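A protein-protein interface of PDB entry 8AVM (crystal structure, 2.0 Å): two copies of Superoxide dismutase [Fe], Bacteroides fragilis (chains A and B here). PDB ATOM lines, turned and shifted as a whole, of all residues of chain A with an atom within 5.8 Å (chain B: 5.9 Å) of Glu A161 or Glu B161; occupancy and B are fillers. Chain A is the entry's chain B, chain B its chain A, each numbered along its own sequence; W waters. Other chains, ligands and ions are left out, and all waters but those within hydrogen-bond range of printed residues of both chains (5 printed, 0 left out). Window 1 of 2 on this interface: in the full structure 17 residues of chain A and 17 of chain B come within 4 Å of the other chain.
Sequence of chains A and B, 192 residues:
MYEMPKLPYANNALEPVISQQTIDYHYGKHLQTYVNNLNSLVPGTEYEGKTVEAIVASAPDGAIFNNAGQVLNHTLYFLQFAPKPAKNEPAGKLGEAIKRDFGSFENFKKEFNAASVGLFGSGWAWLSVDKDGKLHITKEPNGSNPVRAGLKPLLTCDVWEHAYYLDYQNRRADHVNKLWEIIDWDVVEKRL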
ATOM      1  N   HIS A  30     -17.386  21.356  10.032  1.00  0.00           N
ATOM      2  CA  HIS A  30     -16.101  20.659   9.985  1.00  0.00           C
ATOM      3  C   HIS A  30     -16.160  19.445   9.073  1.00  0.00           C
ATOM      4  O   HIS A  30     -15.308  19.299   8.223  1.00  0.00           O
ATOM      5  CB  HIS A  30     -15.605  20.240  11.388  1.00  0.00           C
ATOM      6  CG  HIS A  30     -15.155  21.375  12.272  1.00  0.00           C
ATOM      7  ND1 HIS A  30     -13.851  21.844  12.296  1.00  0.00           N
ATOM      8  CD2 HIS A  30     -15.862  22.140  13.136  1.00  0.00           C
ATOM      9  CE1 HIS A  30     -13.778  22.860  13.160  1.00  0.00           C
ATOM     10  NE2 HIS A  30     -14.990  23.053  13.677  1.00  0.00           N
ATOM     11  N   SER A 122      -4.417  17.685  19.075  1.00  0.00           N
ATOM     12  CA  SER A 122      -5.576  17.220  18.337  1.00  0.00           C
ATOM     13  C   SER A 122      -5.414  15.743  18.001  1.00  0.00           C
ATOM     14  O   SER A 122      -4.323  15.311  17.661  1.00  0.00           O
ATOM     15  CB  SER A 122      -5.788  18.036  17.064  1.00  0.00           C
ATOM     16  OG  SER A 122      -5.957  19.415  17.361  1.00  0.00           O
ATOM     17  N   ASP A 158     -13.322  11.872  19.796  1.00  0.00           N
ATOM     18  CA  ASP A 158     -12.670  12.970  19.101  1.00  0.00           C
ATOM     19  C   ASP A 158     -12.224  13.961  20.166  1.00  0.00           C
ATOM     20  O   ASP A 158     -13.084  14.549  20.834  1.00  0.00           O
ATOM     21  CB  ASP A 158     -13.643  13.661  18.142  1.00  0.00           C
ATOM     22  CG  ASP A 158     -13.081  14.778  17.308  1.00  0.00           C
ATOM     23  OD1 ASP A 158     -11.864  15.070  17.428  1.00  0.00           O
ATOM     24  OD2 ASP A 158     -13.873  15.314  16.494  1.00  0.00           O
ATOM     25  N   VAL A 159     -10.893  14.167  20.296  1.00  0.00           N
ATOM     26  CA  VAL A 159     -10.409  15.118  21.289  1.00  0.00           C
ATOM     27  C   VAL A 159      -9.809  16.359  20.643  1.00  0.00           C
ATOM     28  O   VAL A 159      -9.166  17.151  21.335  1.00  0.00           O
ATOM     29  CB  VAL A 159      -9.432  14.473  22.295  1.00  0.00           C
ATOM     30  CG1 VAL A 159     -10.111  13.365  23.094  1.00  0.00           C
ATOM     31  CG2 VAL A 159      -8.152  13.979  21.645  1.00  0.00           C
ATOM     32  N   TRP A 160     -10.055  16.577  19.344  1.00  0.00           N
ATOM     33  CA  TRP A 160      -9.961  17.915  18.800  1.00  0.00           C
ATOM     34  C   TRP A 160     -10.832  18.811  19.662  1.00  0.00           C
ATOM     35  O   TRP A 160     -11.965  18.466  19.978  1.00  0.00           O
ATOM     36  CB  TRP A 160     -10.427  17.990  17.338  1.00  0.00           C
ATOM     37  CG  TRP A 160      -9.506  17.361  16.340  1.00  0.00           C
ATOM     38  CD1 TRP A 160      -9.144  16.048  16.250  1.00  0.00           C
ATOM     39  CD2 TRP A 160      -8.887  18.030  15.233  1.00  0.00           C
ATOM     40  NE1 TRP A 160      -8.318  15.860  15.177  1.00  0.00           N
ATOM     41  CE2 TRP A 160      -8.164  17.050  14.515  1.00  0.00           C
ATOM     42  CE3 TRP A 160      -8.903  19.344  14.747  1.00  0.00           C
ATOM     43  CZ2 TRP A 160      -7.406  17.371  13.381  1.00  0.00           C
ATOM     44  CZ3 TRP A 160      -8.183  19.659  13.619  1.00  0.00           C
ATOM     45  CH2 TRP A 160      -7.459  18.671  12.922  1.00  0.00           C
ATOM     46  N   GLU A 161     -10.349  19.995  19.979  1.00  0.00           N
ATOM     47  CA  GLU A 161     -11.114  20.918  20.813  1.00  0.00           C
ATOM     48  C   GLU A 161     -12.474  21.274  20.225  1.00  0.00           C
ATOM     49  O   GLU A 161     -13.412  21.466  21.005  1.00  0.00           O
ATOM     50  CB  GLU A 161     -10.268  22.156  21.118  1.00  0.00           C
ATOM     51  CG  GLU A 161      -9.189  21.880  22.132  1.00  0.00           C
ATOM     52  CD  GLU A 161      -8.203  22.993  22.437  1.00  0.00           C
ATOM     53  OE1 GLU A 161      -7.768  23.635  21.509  1.00  0.00           O
ATOM     54  OE2 GLU A 161      -7.820  23.117  23.629  1.00  0.00           O
ATOM     55  N   HIS A 162     -12.602  21.365  18.889  1.00  0.00           N
ATOM     56  CA  HIS A 162     -13.909  21.688  18.306  1.00  0.00           C
ATOM     57  C   HIS A 162     -14.986  20.707  18.745  1.00  0.00           C
ATOM     58  O   HIS A 162     -16.184  21.027  18.698  1.00  0.00           O
ATOM     59  CB  HIS A 162     -13.875  21.771  16.765  1.00  0.00           C
ATOM     60  CG  HIS A 162     -13.553  20.511  16.038  1.00  0.00           C
ATOM     61  ND1 HIS A 162     -12.450  20.425  15.221  1.00  0.00           N
ATOM     62  CD2 HIS A 162     -14.162  19.294  15.990  1.00  0.00           C
ATOM     63  CE1 HIS A 162     -12.418  19.171  14.710  1.00  0.00           C
ATOM     64  NE2 HIS A 162     -13.443  18.477  15.157  1.00  0.00           N
ATOM     65  N   ALA A 163     -14.580  19.510  19.173  1.00  0.00           N
ATOM     66  CA  ALA A 163     -15.560  18.488  19.511  1.00  0.00           C
ATOM     67  C   ALA A 163     -16.278  18.824  20.817  1.00  0.00           C
ATOM     68  O   ALA A 163     -17.390  18.332  21.057  1.00  0.00           O
ATOM     69  CB  ALA A 163     -14.893  17.120  19.613  1.00  0.00           C
ATOM     70  N   TYR A 164     -15.629  19.638  21.668  1.00  0.00           N
ATOM     71  CA  TYR A 164     -16.143  19.883  23.016  1.00  0.00           C
ATOM     72  C   TYR A 164     -16.061  21.330  23.471  1.00  0.00           C
ATOM     73  O   TYR A 164     -16.674  21.669  24.465  1.00  0.00           O
ATOM     74  CB  TYR A 164     -15.431  19.008  24.045  1.00  0.00           C
ATOM     75  CG  TYR A 164     -13.935  19.143  24.147  1.00  0.00           C
ATOM     76  CD1 TYR A 164     -13.329  20.132  24.897  1.00  0.00           C
ATOM     77  CD2 TYR A 164     -13.112  18.231  23.502  1.00  0.00           C
ATOM     78  CE1 TYR A 164     -11.951  20.207  25.035  1.00  0.00           C
ATOM     79  CE2 TYR A 164     -11.727  18.308  23.600  1.00  0.00           C
ATOM     80  CZ  TYR A 164     -11.140  19.303  24.358  1.00  0.00           C
ATOM     81  OH  TYR A 164      -9.745  19.347  24.465  1.00  0.00           O
ATOM     82  N   TYR A 165     -15.364  22.203  22.761  1.00  0.00           N
ATOM     83  CA  TYR A 165     -15.044  23.492  23.335  1.00  0.00           C
ATOM     84  C   TYR A 165     -16.285  24.346  23.555  1.00  0.00           C
ATOM     85  O   TYR A 165     -16.344  25.088  24.534  1.00  0.00           O
ATOM     86  CB  TYR A 165     -13.995  24.253  22.525  1.00  0.00           C
ATOM     87  CG  TYR A 165     -13.088  25.087  23.389  1.00  0.00           C
ATOM     88  CD1 TYR A 165     -12.067  24.484  24.115  1.00  0.00           C
ATOM     89  CD2 TYR A 165     -13.285  26.452  23.561  1.00  0.00           C
ATOM     90  CE1 TYR A 165     -11.281  25.218  24.988  1.00  0.00           C
ATOM     91  CE2 TYR A 165     -12.480  27.199  24.414  1.00  0.00           C
ATOM     92  CZ  TYR A 165     -11.482  26.584  25.146  1.00  0.00           C
ATOM     93  OH  TYR A 165     -10.672  27.280  26.037  1.00  0.00           O
ATOM     94  N   LEU A 166     -17.284  24.279  22.683  1.00  0.00           N
ATOM     95  CA  LEU A 166     -18.453  25.153  22.867  1.00  0.00           C
ATOM     96  C   LEU A 166     -19.257  24.712  24.090  1.00  0.00           C
ATOM     97  O   LEU A 166     -19.933  25.552  24.697  1.00  0.00           O
ATOM     98  CB  LEU A 166     -19.380  25.107  21.645  1.00  0.00           C
ATOM     99  CG  LEU A 166     -18.793  25.646  20.342  1.00  0.00           C
ATOM    100  CD1 LEU A 166     -19.727  25.314  19.181  1.00  0.00           C
ATOM    101  CD2 LEU A 166     -18.497  27.158  20.437  1.00  0.00           C
ATOM    102  N   GLN A 169     -15.582  23.960  27.107  1.00  0.00           N
ATOM    103  CA  GLN A 169     -14.336  24.696  26.997  1.00  0.00           C
ATOM    104  C   GLN A 169     -13.151  23.764  27.246  1.00  0.00           C
ATOM    105  O   GLN A 169     -13.045  22.719  26.611  1.00  0.00           O
ATOM    106  CB  GLN A 169     -14.403  25.922  27.907  1.00  0.00           C
ATOM    107  CG  GLN A 169     -15.485  26.910  27.484  1.00  0.00           C
ATOM    108  CD  GLN A 169     -16.857  26.535  27.996  1.00  0.00           C
ATOM    109  OE1 GLN A 169     -17.051  26.216  29.165  1.00  0.00           O
ATOM    110  NE2 GLN A 169     -17.817  26.513  27.102  1.00  0.00           N
ATOM    111  N   ASN A 170     -12.262  24.136  28.174  1.00  0.00           N
ATOM    112  CA  ASN A 170     -11.042  23.372  28.415  1.00  0.00           C
ATOM    113  C   ASN A 170     -11.290  22.064  29.161  1.00  0.00           C
ATOM    114  O   ASN A 170     -10.349  21.323  29.397  1.00  0.00           O
ATOM    115  CB  ASN A 170     -10.013  24.183  29.219  1.00  0.00           C
ATOM    116  CG  ASN A 170     -10.536  24.613  30.571  1.00  0.00           C
ATOM    117  OD1 ASN A 170     -11.609  25.201  30.692  1.00  0.00           O
ATOM    118  ND2 ASN A 170      -9.783  24.322  31.607  1.00  0.00           N
ATOM    119  N   ARG A 172     -11.893  18.892  28.971  1.00  0.00           N
ATOM    120  CA  ARG A 172     -11.968  17.710  28.129  1.00  0.00           C
ATOM    121  C   ARG A 172     -12.438  16.490  28.912  1.00  0.00           C
ATOM    122  O   ARG A 172     -13.279  15.722  28.432  1.00  0.00           O
ATOM    123  CB  ARG A 172     -10.601  17.406  27.498  1.00  0.00           C
ATOM    124  CG  ARG A 172     -10.669  16.250  26.492  1.00  0.00           C
ATOM    125  CD  ARG A 172      -9.312  15.750  26.059  1.00  0.00           C
ATOM    126  NE  ARG A 172      -8.588  16.701  25.229  1.00  0.00           N
ATOM    127  CZ  ARG A 172      -7.382  16.467  24.737  1.00  0.00           C
ATOM    128  NH1 ARG A 172      -6.782  17.350  23.961  1.00  0.00           N
ATOM    129  NH2 ARG A 172      -6.859  15.283  24.947  1.00  0.00           N
ATOM    130  N   HIS B  30      -6.125  27.745  30.373  1.00  0.00           N
ATOM    131  CA  HIS B  30      -5.146  26.953  29.632  1.00  0.00           C
ATOM    132  C   HIS B  30      -3.727  27.298  30.088  1.00  0.00           C
ATOM    133  O   HIS B  30      -2.933  26.393  30.401  1.00  0.00           O
ATOM    134  CB  HIS B  30      -5.303  27.116  28.114  1.00  0.00           C
ATOM    135  CG  HIS B  30      -6.501  26.492  27.500  1.00  0.00           C
ATOM    136  ND1 HIS B  30      -6.583  25.206  27.002  1.00  0.00           N
ATOM    137  CD2 HIS B  30      -7.713  27.073  27.240  1.00  0.00           C
ATOM    138  CE1 HIS B  30      -7.816  24.979  26.547  1.00  0.00           C
ATOM    139  NE2 HIS B  30      -8.529  26.118  26.678  1.00  0.00           N
ATOM    140  N   GLY B 121      -4.296  20.535  12.478  1.00  0.00           N
ATOM    141  CA  GLY B 121      -4.282  20.187  13.895  1.00  0.00           C
ATOM    142  C   GLY B 121      -3.878  21.397  14.763  1.00  0.00           C
ATOM    143  O   GLY B 121      -4.195  22.543  14.446  1.00  0.00           O
ATOM    144  N   SER B 122      -3.271  21.088  15.918  1.00  0.00           N
ATOM    145  CA  SER B 122      -2.870  22.043  16.932  1.00  0.00           C
ATOM    146  C   SER B 122      -1.419  22.448  16.680  1.00  0.00           C
ATOM    147  O   SER B 122      -0.579  21.632  16.326  1.00  0.00           O
ATOM    148  CB  SER B 122      -3.041  21.470  18.323  1.00  0.00           C
ATOM    149  OG  SER B 122      -4.423  21.083  18.559  1.00  0.00           O
ATOM    150  N   ASP B 158      -1.311  31.346  17.508  1.00  0.00           N
ATOM    151  CA  ASP B 158      -1.725  30.111  18.136  1.00  0.00           C
ATOM    152  C   ASP B 158      -2.911  29.586  17.356  1.00  0.00           C
ATOM    153  O   ASP B 158      -3.959  30.248  17.349  1.00  0.00           O
ATOM    154  CB  ASP B 158      -2.177  30.345  19.585  1.00  0.00           C
ATOM    155  CG  ASP B 158      -2.581  29.126  20.384  1.00  0.00           C
ATOM    156  OD1 ASP B 158      -2.490  28.005  19.830  1.00  0.00           O
ATOM    157  OD2 ASP B 158      -2.921  29.300  21.560  1.00  0.00           O
ATOM    158  N   VAL B 159      -2.753  28.410  16.719  1.00  0.00           N
ATOM    159  CA  VAL B 159      -3.851  27.868  15.932  1.00  0.00           C
ATOM    160  C   VAL B 159      -4.467  26.631  16.583  1.00  0.00           C
ATOM    161  O   VAL B 159      -5.290  25.974  15.948  1.00  0.00           O
ATOM    162  CB  VAL B 159      -3.479  27.617  14.458  1.00  0.00           C
ATOM    163  CG1 VAL B 159      -3.103  28.894  13.754  1.00  0.00           C
ATOM    164  CG2 VAL B 159      -2.406  26.561  14.299  1.00  0.00           C
ATOM    165  N   TRP B 160      -4.130  26.355  17.851  1.00  0.00           N
ATOM    166  CA  TRP B 160      -4.971  25.519  18.668  1.00  0.00           C
ATOM    167  C   TRP B 160      -6.379  26.103  18.600  1.00  0.00           C
ATOM    168  O   TRP B 160      -6.576  27.314  18.697  1.00  0.00           O
ATOM    169  CB  TRP B 160      -4.501  25.479  20.126  1.00  0.00           C
ATOM    170  CG  TRP B 160      -3.249  24.707  20.393  1.00  0.00           C
ATOM    171  CD1 TRP B 160      -2.007  24.945  19.887  1.00  0.00           C
ATOM    172  CD2 TRP B 160      -3.126  23.577  21.256  1.00  0.00           C
ATOM    173  NE1 TRP B 160      -1.121  24.046  20.388  1.00  0.00           N
ATOM    174  CE2 TRP B 160      -1.768  23.194  21.236  1.00  0.00           C
ATOM    175  CE3 TRP B 160      -4.017  22.858  22.069  1.00  0.00           C
ATOM    176  CZ2 TRP B 160      -1.298  22.088  21.954  1.00  0.00           C
ATOM    177  CZ3 TRP B 160      -3.543  21.809  22.833  1.00  0.00           C
ATOM    178  CH2 TRP B 160      -2.203  21.415  22.759  1.00  0.00           C
ATOM    179  N   GLU B 161      -7.365  25.236  18.499  1.00  0.00           N
ATOM    180  CA  GLU B 161      -8.738  25.739  18.323  1.00  0.00           C
ATOM    181  C   GLU B 161      -9.211  26.602  19.506  1.00  0.00           C
ATOM    182  O   GLU B 161      -9.991  27.540  19.325  1.00  0.00           O
ATOM    183  CB  GLU B 161      -9.673  24.563  18.052  1.00  0.00           C
ATOM    184  CG  GLU B 161      -9.481  24.023  16.620  1.00  0.00           C
ATOM    185  CD  GLU B 161     -10.280  22.777  16.276  1.00  0.00           C
ATOM    186  OE1 GLU B 161     -10.383  21.855  17.126  1.00  0.00           O
ATOM    187  OE2 GLU B 161     -10.880  22.774  15.206  1.00  0.00           O
ATOM    188  N   HIS B 162      -8.761  26.279  20.731  1.00  0.00           N
ATOM    189  CA  HIS B 162      -9.144  27.058  21.900  1.00  0.00           C
ATOM    190  C   HIS B 162      -8.823  28.541  21.721  1.00  0.00           C
ATOM    191  O   HIS B 162      -9.423  29.382  22.398  1.00  0.00           O
ATOM    192  CB  HIS B 162      -8.507  26.515  23.194  1.00  0.00           C
ATOM    193  CG  HIS B 162      -7.017  26.642  23.292  1.00  0.00           C
ATOM    194  ND1 HIS B 162      -6.244  25.528  23.493  1.00  0.00           N
ATOM    195  CD2 HIS B 162      -6.160  27.680  23.261  1.00  0.00           C
ATOM    196  CE1 HIS B 162      -4.974  25.902  23.567  1.00  0.00           C
ATOM    197  NE2 HIS B 162      -4.885  27.191  23.430  1.00  0.00           N
ATOM    198  N   ALA B 163      -7.896  28.863  20.806  1.00  0.00           N
ATOM    199  CA  ALA B 163      -7.444  30.247  20.690  1.00  0.00           C
ATOM    200  C   ALA B 163      -8.529  31.098  20.019  1.00  0.00           C
ATOM    201  O   ALA B 163      -8.543  32.335  20.162  1.00  0.00           O
ATOM    202  CB  ALA B 163      -6.123  30.312  19.921  1.00  0.00           C
ATOM    203  N   TYR B 164      -9.388  30.444  19.228  1.00  0.00           N
ATOM    204  CA  TYR B 164     -10.344  31.155  18.392  1.00  0.00           C
ATOM    205  C   TYR B 164     -11.761  30.578  18.406  1.00  0.00           C
ATOM    206  O   TYR B 164     -12.692  31.214  17.912  1.00  0.00           O
ATOM    207  CB  TYR B 164      -9.833  31.231  16.953  1.00  0.00           C
ATOM    208  CG  TYR B 164      -9.573  29.939  16.230  1.00  0.00           C
ATOM    209  CD1 TYR B 164     -10.587  29.209  15.611  1.00  0.00           C
ATOM    210  CD2 TYR B 164      -8.285  29.423  16.155  1.00  0.00           C
ATOM    211  CE1 TYR B 164     -10.323  28.030  14.916  1.00  0.00           C
ATOM    212  CE2 TYR B 164      -8.020  28.227  15.492  1.00  0.00           C
ATOM    213  CZ  TYR B 164      -9.022  27.528  14.867  1.00  0.00           C
ATOM    214  OH  TYR B 164      -8.706  26.357  14.143  1.00  0.00           O
ATOM    215  N   TYR B 165     -11.967  29.389  18.940  1.00  0.00           N
ATOM    216  CA  TYR B 165     -13.229  28.709  18.654  1.00  0.00           C
ATOM    217  C   TYR B 165     -14.423  29.446  19.265  1.00  0.00           C
ATOM    218  O   TYR B 165     -15.506  29.447  18.685  1.00  0.00           O
ATOM    219  CB  TYR B 165     -13.209  27.246  19.108  1.00  0.00           C
ATOM    220  CG  TYR B 165     -14.046  26.371  18.208  1.00  0.00           C
ATOM    221  CD1 TYR B 165     -13.582  26.002  16.967  1.00  0.00           C
ATOM    222  CD2 TYR B 165     -15.334  25.975  18.566  1.00  0.00           C
ATOM    223  CE1 TYR B 165     -14.354  25.245  16.102  1.00  0.00           C
ATOM    224  CE2 TYR B 165     -16.105  25.187  17.727  1.00  0.00           C
ATOM    225  CZ  TYR B 165     -15.621  24.844  16.467  1.00  0.00           C
ATOM    226  OH  TYR B 165     -16.343  24.078  15.559  1.00  0.00           O
ATOM    227  N   LEU B 166     -14.265  30.050  20.447  1.00  0.00           N
ATOM    228  CA  LEU B 166     -15.382  30.712  21.093  1.00  0.00           C
ATOM    229  C   LEU B 166     -15.817  31.926  20.283  1.00  0.00           C
ATOM    230  O   LEU B 166     -16.997  32.294  20.324  1.00  0.00           O
ATOM    231  CB  LEU B 166     -15.053  31.131  22.531  1.00  0.00           C
ATOM    232  CG  LEU B 166     -14.720  29.999  23.512  1.00  0.00           C
ATOM    233  CD1 LEU B 166     -14.216  30.578  24.821  1.00  0.00           C
ATOM    234  CD2 LEU B 166     -15.956  29.122  23.753  1.00  0.00           C
ATOM    235  N   GLN B 169     -15.482  30.058  15.846  1.00  0.00           N
ATOM    236  CA  GLN B 169     -15.729  28.654  15.604  1.00  0.00           C
ATOM    237  C   GLN B 169     -14.725  28.126  14.587  1.00  0.00           C
ATOM    238  O   GLN B 169     -13.500  28.308  14.771  1.00  0.00           O
ATOM    239  CB  GLN B 169     -17.198  28.478  15.206  1.00  0.00           C
ATOM    240  CG  GLN B 169     -18.167  28.858  16.306  1.00  0.00           C
ATOM    241  CD  GLN B 169     -18.422  30.343  16.403  1.00  0.00           C
ATOM    242  OE1 GLN B 169     -18.704  31.035  15.433  1.00  0.00           O
ATOM    243  NE2 GLN B 169     -18.291  30.863  17.603  1.00  0.00           N
ATOM    244  N   ARG B 172     -11.002  29.703  11.096  1.00  0.00           N
ATOM    245  CA  ARG B 172      -9.636  30.039  11.495  1.00  0.00           C
ATOM    246  C   ARG B 172      -9.076  31.200  10.687  1.00  0.00           C
ATOM    247  O   ARG B 172      -8.415  32.104  11.261  1.00  0.00           O
ATOM    248  CB  ARG B 172      -8.720  28.828  11.390  1.00  0.00           C
ATOM    249  CG  ARG B 172      -7.318  29.097  11.918  1.00  0.00           C
ATOM    250  CD  ARG B 172      -6.252  28.076  11.550  1.00  0.00           C
ATOM    251  NE  ARG B 172      -6.435  26.825  12.244  1.00  0.00           N
ATOM    252  CZ  ARG B 172      -5.631  25.775  12.057  1.00  0.00           C
ATOM    253  NH1 ARG B 172      -5.823  24.644  12.725  1.00  0.00           N
ATOM    254  NH2 ARG B 172      -4.574  25.929  11.268  1.00  0.00           N
HETATM  255  O   HOH W   1     -17.594  21.872  16.654  1.00  0.00           O
HETATM  256  O   HOH W   2      -9.726  29.728  25.066  1.00  0.00           O
HETATM  257  O   HOH W   3      -8.231  20.618  18.142  1.00  0.00           O
HETATM  258  O   HOH W   4      -6.570  22.629  19.146  1.00  0.00           O
HETATM  259  O   HOH W   5      -2.493  18.434  17.076  1.00  0.00           O
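Among the printed residues, merely in contact across the chains: His A30 with Glu B161, Ser A122 with Gly B121, Trp A160 with Gly B121, Trp A160 with Glu B161, Glu A161 with His B30, Glu A161 with Trp B160, His A162 with Tyr B165, Tyr A165 with His B162, Tyr A165 with Leu B166, Leu A166 with Tyr B165 and Asn A170 with His B30.
His A30 touches Tyr B165, and with the chains exchanged Tyr A165 touches His B30. Ser A122 touches its own counterpart, Ser B122. Glu B161 touches its own counterpart, Glu A161. Glu A161 touches His B162, and with the chains exchanged His A162 touches Glu B161. 13 positions are printed for both chains.
Along chain B the printed residues that touch a printed residue of chain A span positions 30 to 166. Printed residues of chain A that touch a printed residue of chain B: His A30, Ser A122, Trp A160, Glu A161, His A162, Tyr A165, Leu A166 and Asn A170. Along chain A the printed residues that touch a printed residue of chain B span positions 30 to 170. Among the printed residues, 17 pairs touch across the chains.
NE2 of Gln B169 lies within hydrogen-bond range of O of Leu B166. The side-chain amide nitrogen (NE2) of Gln A169 sits close to the backbone carbonyl oxygen (O) of Tyr A165, at 3.3 Å. The guanidinium group (NH1) of Arg B172 lies within hydrogen-bond range of the backbone carbonyl oxygen (O) of Gly B121, at 3.2 Å. NE2 of Gln A169 lies within hydrogen-bond range of O of Leu A166 (3.3 Å). The side-chain carboxylate (OD1) of Asp B158 sits at hydrogen-bond distance from the backbone NH (N) of Trp B160. OD1 of Asp A158 is in hydrogen-bond range of N of Trp A160 (3.0 Å).
The side-chain carboxylate of Glu B161 lies within hydrogen-bond range of a ring nitrogen (ND1) of His A162. A ring nitrogen (ND1) of His B162 lies within hydrogen-bond range of the side-chain carboxylate (OE2) of Glu A161 (2.9 Å). OG of Ser A122 is in hydrogen-bond range of OG of Ser B122. NE2 of His A30 sits at hydrogen-bond distance from OH of Tyr B165 (2.5 Å). The backbone NH (N) of Glu A161 is in hydrogen-bond range of the side-chain carboxylate (OE1) of Glu B161, 3.4 Å away. The side-chain hydroxyl (OH) of Tyr A165 is in hydrogen-bond range of a ring nitrogen (NE2) of His B30, 2.5 Å away.
Printed residues of chain A within 4 Å of Trp B160: Glu A161. Of chain A, only His A30, Trp A160, Glu A161 and His A162 come within 4 Å of Glu B161. Of the printed residues of chain A, His B162 touches Glu A161 (2.9 Å) and Tyr A165 (3.5 Å). Printed residues of chain A within 4 Å of Tyr B165: His A30 (2.5 Å), His A162 (3.5 Å) and Leu A166 (3.8 Å). The nearest residue of chain B that does not touch Glu A161 is Ser B122 (5.1 Å). The nearest residue of chain A that does not touch Glu B161 is Ser A122 (5.1 Å).
Water W1 bridges O of His A162 (2.6 Å) and OH of Tyr B165 (2.8 Å). Water W3 lies within hydrogen-bond range of OE1 of Glu B161, OG of Ser A122 and N of Glu A161. Water W2 lies within hydrogen-bond range of the backbone carbonyl oxygen of His B162 (2.7 Å) and the side-chain hydroxyl of Tyr A165 (2.8 Å). Water W4 lies within hydrogen-bond range of the side-chain hydroxyl (OG) of Ser B122 (2.7 Å), the backbone NH (N) of Glu B161 (2.8 Å) and the side-chain carboxylate (OE1) of Glu A161 (2.8 Å). Water W5 bridges N of Ser A122 (2.9 Å) and N of Ser B122 (3.0 Å).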
